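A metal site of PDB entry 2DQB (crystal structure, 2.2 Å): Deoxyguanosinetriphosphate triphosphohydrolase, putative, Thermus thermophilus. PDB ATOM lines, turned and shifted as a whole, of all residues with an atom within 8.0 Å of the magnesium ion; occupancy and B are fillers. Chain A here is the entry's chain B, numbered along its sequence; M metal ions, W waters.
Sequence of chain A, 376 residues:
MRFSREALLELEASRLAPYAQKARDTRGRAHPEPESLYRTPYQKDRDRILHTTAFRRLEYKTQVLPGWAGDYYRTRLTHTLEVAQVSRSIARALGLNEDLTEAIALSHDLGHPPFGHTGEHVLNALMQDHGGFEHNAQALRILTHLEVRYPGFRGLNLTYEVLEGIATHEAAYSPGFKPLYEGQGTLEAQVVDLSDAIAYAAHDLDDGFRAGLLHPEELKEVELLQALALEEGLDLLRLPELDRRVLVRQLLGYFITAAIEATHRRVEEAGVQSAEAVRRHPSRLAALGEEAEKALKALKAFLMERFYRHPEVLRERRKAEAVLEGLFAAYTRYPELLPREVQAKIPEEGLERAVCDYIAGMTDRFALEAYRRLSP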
ATOM      1  N   VAL A  83      15.774  -3.928  -7.878  1.00  0.00           N
ATOM      2  CA  VAL A  83      15.084  -3.124  -8.868  1.00  0.00           C
ATOM      3  C   VAL A  83      14.769  -1.735  -8.318  1.00  0.00           C
ATOM      4  O   VAL A  83      14.810  -0.717  -9.023  1.00  0.00           O
ATOM      5  CB  VAL A  83      13.736  -3.768  -9.289  1.00  0.00           C
ATOM      6  CG1 VAL A  83      12.950  -2.778 -10.133  1.00  0.00           C
ATOM      7  CG2 VAL A  83      13.991  -5.039 -10.068  1.00  0.00           C
ATOM      8  N   ILE A 104       6.572   2.207  -7.501  1.00  0.00           N
ATOM      9  CA  ILE A 104       6.308   1.342  -8.626  1.00  0.00           C
ATOM     10  C   ILE A 104       7.217   0.110  -8.635  1.00  0.00           C
ATOM     11  O   ILE A 104       6.768  -0.993  -8.945  1.00  0.00           O
ATOM     12  CB  ILE A 104       6.450   2.150  -9.974  1.00  0.00           C
ATOM     13  CG1 ILE A 104       5.470   3.319  -9.971  1.00  0.00           C
ATOM     14  CG2 ILE A 104       6.202   1.258 -11.165  1.00  0.00           C
ATOM     15  CD1 ILE A 104       5.604   4.269 -11.151  1.00  0.00           C
ATOM     16  N   ALA A 105       8.488   0.273  -8.260  1.00  0.00           N
ATOM     17  CA  ALA A 105       9.408  -0.866  -8.236  1.00  0.00           C
ATOM     18  C   ALA A 105       8.996  -1.865  -7.152  1.00  0.00           C
ATOM     19  O   ALA A 105       9.166  -3.084  -7.280  1.00  0.00           O
ATOM     20  CB  ALA A 105      10.845  -0.358  -7.965  1.00  0.00           C
ATOM     21  N   SER A 107       5.781  -2.255  -5.982  1.00  0.00           N
ATOM     22  CA  SER A 107       4.460  -2.810  -6.321  1.00  0.00           C
ATOM     23  C   SER A 107       4.373  -3.677  -7.601  1.00  0.00           C
ATOM     24  O   SER A 107       3.705  -4.711  -7.609  1.00  0.00           O
ATOM     25  CB  SER A 107       3.460  -1.692  -6.454  1.00  0.00           C
ATOM     26  OG  SER A 107       3.752  -0.921  -7.602  1.00  0.00           O
ATOM     27  N   HIS A 108       5.006  -3.223  -8.686  1.00  0.00           N
ATOM     28  CA  HIS A 108       5.002  -3.982  -9.935  1.00  0.00           C
ATOM     29  C   HIS A 108       5.512  -5.317  -9.424  1.00  0.00           C
ATOM     30  O   HIS A 108       6.189  -5.333  -8.403  1.00  0.00           O
ATOM     31  CB  HIS A 108       5.983  -3.360 -10.951  1.00  0.00           C
ATOM     32  CG  HIS A 108       7.360  -3.946 -10.894  1.00  0.00           C
ATOM     33  ND1 HIS A 108       7.953  -4.544 -11.990  1.00  0.00           N
ATOM     34  CD2 HIS A 108       8.213  -4.130  -9.869  1.00  0.00           C
ATOM     35  CE1 HIS A 108       9.104  -5.083 -11.634  1.00  0.00           C
ATOM     36  NE2 HIS A 108       9.287  -4.846 -10.346  1.00  0.00           N
ATOM     37  N   ASP A 109       5.206  -6.418 -10.067  1.00  0.00           N
ATOM     38  CA  ASP A 109       5.674  -7.727  -9.556  1.00  0.00           C
ATOM     39  C   ASP A 109       4.928  -8.369  -8.376  1.00  0.00           C
ATOM     40  O   ASP A 109       5.165  -9.511  -8.058  1.00  0.00           O
ATOM     41  CB  ASP A 109       7.143  -7.663  -9.175  1.00  0.00           C
ATOM     42  CG  ASP A 109       8.014  -8.171 -10.283  1.00  0.00           C
ATOM     43  OD1 ASP A 109       7.506  -8.283 -11.420  1.00  0.00           O
ATOM     44  OD2 ASP A 109       9.202  -8.456 -10.010  1.00  0.00           O
ATOM     45  N   LEU A 110       4.053  -7.625  -7.730  1.00  0.00           N
ATOM     46  CA  LEU A 110       3.274  -8.205  -6.622  1.00  0.00           C
ATOM     47  C   LEU A 110       2.342  -9.301  -7.154  1.00  0.00           C
ATOM     48  O   LEU A 110       1.916 -10.174  -6.402  1.00  0.00           O
ATOM     49  CB  LEU A 110       2.422  -7.114  -5.969  1.00  0.00           C
ATOM     50  CG  LEU A 110       2.698  -6.627  -4.550  1.00  0.00           C
ATOM     51  CD1 LEU A 110       4.133  -6.886  -4.145  1.00  0.00           C
ATOM     52  CD2 LEU A 110       2.345  -5.151  -4.498  1.00  0.00           C
ATOM     53  N   HIS A 112       2.816 -11.924  -9.325  1.00  0.00           N
ATOM     54  CA  HIS A 112       3.329 -13.167  -9.838  1.00  0.00           C
ATOM     55  C   HIS A 112       2.867 -14.348  -8.970  1.00  0.00           C
ATOM     56  O   HIS A 112       2.715 -14.224  -7.760  1.00  0.00           O
ATOM     57  CB  HIS A 112       4.867 -13.137  -9.886  1.00  0.00           C
ATOM     58  CG  HIS A 112       5.429 -12.546 -11.144  1.00  0.00           C
ATOM     59  ND1 HIS A 112       5.946 -11.271 -11.198  1.00  0.00           N
ATOM     60  CD2 HIS A 112       5.509 -13.043 -12.397  1.00  0.00           C
ATOM     61  CE1 HIS A 112       6.324 -11.016 -12.441  1.00  0.00           C
ATOM     62  NE2 HIS A 112       6.068 -12.066 -13.189  1.00  0.00           N
ATOM     63  N   GLU A 134      -2.486 -12.494 -16.256  1.00  0.00           N
ATOM     64  CA  GLU A 134      -1.343 -11.661 -16.621  1.00  0.00           C
ATOM     65  C   GLU A 134      -0.843 -10.973 -15.331  1.00  0.00           C
ATOM     66  O   GLU A 134      -1.616 -10.322 -14.629  1.00  0.00           O
ATOM     67  CB  GLU A 134      -1.788 -10.654 -17.686  1.00  0.00           C
ATOM     68  CG  GLU A 134      -0.651 -10.198 -18.595  1.00  0.00           C
ATOM     69  CD  GLU A 134       0.308  -9.242 -17.904  1.00  0.00           C
ATOM     70  OE1 GLU A 134       1.537  -9.468 -18.010  1.00  0.00           O
ATOM     71  OE2 GLU A 134      -0.180  -8.271 -17.278  1.00  0.00           O
ATOM     72  N   HIS A 135       0.444 -11.137 -15.002  1.00  0.00           N
ATOM     73  CA  HIS A 135       1.018 -10.611 -13.762  1.00  0.00           C
ATOM     74  C   HIS A 135       0.829  -9.124 -13.438  1.00  0.00           C
ATOM     75  O   HIS A 135       0.600  -8.789 -12.274  1.00  0.00           O
ATOM     76  CB  HIS A 135       2.496 -11.016 -13.620  1.00  0.00           C
ATOM     77  CG  HIS A 135       3.468 -10.056 -14.247  1.00  0.00           C
ATOM     78  ND1 HIS A 135       3.732 -10.039 -15.600  1.00  0.00           N
ATOM     79  CD2 HIS A 135       4.239  -9.084 -13.698  1.00  0.00           C
ATOM     80  CE1 HIS A 135       4.637  -9.115 -15.857  1.00  0.00           C
ATOM     81  NE2 HIS A 135       4.960  -8.520 -14.722  1.00  0.00           N
ATOM     82  N   ASN A 136       0.897  -8.230 -14.421  1.00  0.00           N
ATOM     83  CA  ASN A 136       0.686  -6.814 -14.115  1.00  0.00           C
ATOM     84  C   ASN A 136      -0.790  -6.588 -13.795  1.00  0.00           C
ATOM     85  O   ASN A 136      -1.118  -5.840 -12.883  1.00  0.00           O
ATOM     86  CB  ASN A 136       1.108  -5.917 -15.294  1.00  0.00           C
ATOM     87  CG  ASN A 136       2.593  -6.058 -15.604  1.00  0.00           C
ATOM     88  OD1 ASN A 136       2.958  -6.619 -16.639  1.00  0.00           O
ATOM     89  ND2 ASN A 136       3.441  -5.580 -14.700  1.00  0.00           N
ATOM     90  N   ALA A 139      -1.351  -7.747 -10.379  1.00  0.00           N
ATOM     91  CA  ALA A 139      -0.848  -6.779  -9.431  1.00  0.00           C
ATOM     92  C   ALA A 139      -1.914  -5.717  -9.169  1.00  0.00           C
ATOM     93  O   ALA A 139      -2.221  -5.381  -8.017  1.00  0.00           O
ATOM     94  CB  ALA A 139       0.405  -6.108  -9.984  1.00  0.00           C
ATOM     95  N   GLY A 165       1.536   3.463 -13.313  1.00  0.00           N
ATOM     96  CA  GLY A 165       2.859   2.940 -13.620  1.00  0.00           C
ATOM     97  C   GLY A 165       2.896   1.453 -13.804  1.00  0.00           C
ATOM     98  O   GLY A 165       3.574   0.925 -14.698  1.00  0.00           O
ATOM     99  N   ILE A 166       2.149   0.735 -12.961  1.00  0.00           N
ATOM    100  CA  ILE A 166       2.140  -0.730 -13.011  1.00  0.00           C
ATOM    101  C   ILE A 166       1.646  -1.307 -14.340  1.00  0.00           C
ATOM    102  O   ILE A 166       0.768  -0.734 -14.975  1.00  0.00           O
ATOM    103  CB  ILE A 166       1.289  -1.275 -11.836  1.00  0.00           C
ATOM    104  CG1 ILE A 166       2.026  -0.996 -10.516  1.00  0.00           C
ATOM    105  CG2 ILE A 166       0.990  -2.737 -12.058  1.00  0.00           C
ATOM    106  CD1 ILE A 166       1.316  -1.433  -9.229  1.00  0.00           C
ATOM    107  N   HIS A 169       4.143   0.677 -17.203  1.00  0.00           N
ATOM    108  CA  HIS A 169       5.599   0.511 -17.240  1.00  0.00           C
ATOM    109  C   HIS A 169       5.692  -0.837 -17.937  1.00  0.00           C
ATOM    110  O   HIS A 169       4.774  -1.654 -17.789  1.00  0.00           O
ATOM    111  CB  HIS A 169       6.188   0.370 -15.843  1.00  0.00           C
ATOM    112  CG  HIS A 169       6.076  -1.017 -15.297  1.00  0.00           C
ATOM    113  ND1 HIS A 169       4.867  -1.612 -14.986  1.00  0.00           N
ATOM    114  CD2 HIS A 169       7.021  -1.965 -15.084  1.00  0.00           C
ATOM    115  CE1 HIS A 169       5.071  -2.859 -14.598  1.00  0.00           C
ATOM    116  NE2 HIS A 169       6.376  -3.104 -14.650  1.00  0.00           N
ATOM    117  N   GLU A 170       6.765  -1.062 -18.700  1.00  0.00           N
ATOM    118  CA  GLU A 170       6.974  -2.323 -19.402  1.00  0.00           C
ATOM    119  C   GLU A 170       6.652  -2.181 -20.884  1.00  0.00           C
ATOM    120  O   GLU A 170       7.547  -2.280 -21.740  1.00  0.00           O
ATOM    121  CB  GLU A 170       6.129  -3.461 -18.792  1.00  0.00           C
ATOM    122  CG  GLU A 170       6.923  -4.753 -18.525  1.00  0.00           C
ATOM    123  CD  GLU A 170       6.120  -5.853 -17.816  1.00  0.00           C
ATOM    124  OE1 GLU A 170       5.203  -6.423 -18.439  1.00  0.00           O
ATOM    125  OE2 GLU A 170       6.413  -6.149 -16.619  1.00  0.00           O
ATOM    126  N   ALA A 189       7.860   5.523 -14.388  1.00  0.00           N
ATOM    127  CA  ALA A 189       7.401   4.162 -14.648  1.00  0.00           C
ATOM    128  C   ALA A 189       8.323   3.444 -15.635  1.00  0.00           C
ATOM    129  O   ALA A 189       8.743   2.297 -15.403  1.00  0.00           O
ATOM    130  CB  ALA A 189       5.985   4.200 -15.202  1.00  0.00           C
ATOM    131  N   VAL A 192      11.498   2.121 -14.107  1.00  0.00           N
ATOM    132  CA  VAL A 192      11.383   0.897 -13.314  1.00  0.00           C
ATOM    133  C   VAL A 192      11.520  -0.324 -14.246  1.00  0.00           C
ATOM    134  O   VAL A 192      12.308  -1.222 -13.972  1.00  0.00           O
ATOM    135  CB  VAL A 192      10.039   0.876 -12.509  1.00  0.00           C
ATOM    136  CG1 VAL A 192       9.898  -0.395 -11.708  1.00  0.00           C
ATOM    137  CG2 VAL A 192       9.976   2.053 -11.580  1.00  0.00           C
ATOM    138  N   ASP A 193      10.829  -0.337 -15.381  1.00  0.00           N
ATOM    139  CA  ASP A 193      10.931  -1.482 -16.293  1.00  0.00           C
ATOM    140  C   ASP A 193      12.353  -1.671 -16.853  1.00  0.00           C
ATOM    141  O   ASP A 193      12.813  -2.785 -17.056  1.00  0.00           O
ATOM    142  CB  ASP A 193       9.910  -1.345 -17.430  1.00  0.00           C
ATOM    143  CG  ASP A 193       9.878  -2.570 -18.368  1.00  0.00           C
ATOM    144  OD1 ASP A 193       9.715  -3.714 -17.894  1.00  0.00           O
ATOM    145  OD2 ASP A 193       9.998  -2.378 -19.596  1.00  0.00           O
ATOM    146  N   ASP A 196      14.416  -3.121 -14.006  1.00  0.00           N
ATOM    147  CA  ASP A 196      14.065  -4.520 -13.761  1.00  0.00           C
ATOM    148  C   ASP A 196      14.888  -5.422 -14.688  1.00  0.00           C
ATOM    149  O   ASP A 196      15.411  -6.466 -14.270  1.00  0.00           O
ATOM    150  CB  ASP A 196      12.552  -4.690 -14.008  1.00  0.00           C
ATOM    151  CG  ASP A 196      12.071  -6.118 -13.875  1.00  0.00           C
ATOM    152  OD1 ASP A 196      12.738  -6.931 -13.217  1.00  0.00           O
ATOM    153  OD2 ASP A 196      10.988  -6.428 -14.409  1.00  0.00           O
ATOM    154  N   TYR A 200      17.697  -8.015 -13.682  1.00  0.00           N
ATOM    155  CA  TYR A 200      17.572  -9.398 -14.125  1.00  0.00           C
ATOM    156  C   TYR A 200      18.871  -9.988 -14.689  1.00  0.00           C
ATOM    157  O   TYR A 200      19.341 -11.039 -14.240  1.00  0.00           O
ATOM    158  CB  TYR A 200      16.502  -9.488 -15.206  1.00  0.00           C
ATOM    159  CG  TYR A 200      15.331 -10.346 -14.841  1.00  0.00           C
ATOM    160  CD1 TYR A 200      14.145  -9.776 -14.377  1.00  0.00           C
ATOM    161  CD2 TYR A 200      15.413 -11.732 -14.937  1.00  0.00           C
ATOM    162  CE1 TYR A 200      13.061 -10.566 -14.023  1.00  0.00           C
ATOM    163  CE2 TYR A 200      14.327 -12.536 -14.582  1.00  0.00           C
ATOM    164  CZ  TYR A 200      13.160 -11.940 -14.131  1.00  0.00           C
ATOM    165  OH  TYR A 200      12.080 -12.719 -13.812  1.00  0.00           O
HETATM  166 MG    MG M   1       7.106  -5.318 -14.234  1.00  0.00          MG
HETATM  167  O   HOH W   1       8.029  -7.143 -13.948  1.00  0.00           O
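ND1 of His 169 sits at hydrogen-bond distance from O of Gly 165.
OE1 of Glu 170 sits close to OD1 of Asn 136, 2.9 Å away.
The side-chain carboxylate of Glu 170 lies close to a ring nitrogen (NE2) of His 135 (3.4 Å).
ND2 of Asn 136 is in hydrogen-bond range of NE2 of His 135 (3.3 Å).
OE2 of Glu 134 lies within hydrogen-bond range of N of Asn 136 (3.1 Å).
ND1 of His 135 sits at hydrogen-bond distance from OE1 of Glu 134, 3.3 Å away.
Merely in contact with the magnesium ion: His 135 and Asn 136.
Five residues have an atom within 4 Å of the magnesium ion: His 108, His 135, Asn 136, His 169 and Glu 170.
The magnesium ion is bound by water W1, a ring nitrogen (NE2) of His 169, a ring nitrogen (ND1) of His 108 and the side-chain carboxylate of Glu 170.
The magnesium ion has four donor atoms within binding distance.
Water W1 lies within hydrogen-bond range of the side-chain carboxylate of Asp 109 (2.8 Å), the side-chain carboxylate of Asp 196 (3.1 Å) and a ring nitrogen (NE2) of His 135 (3.5 Å).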
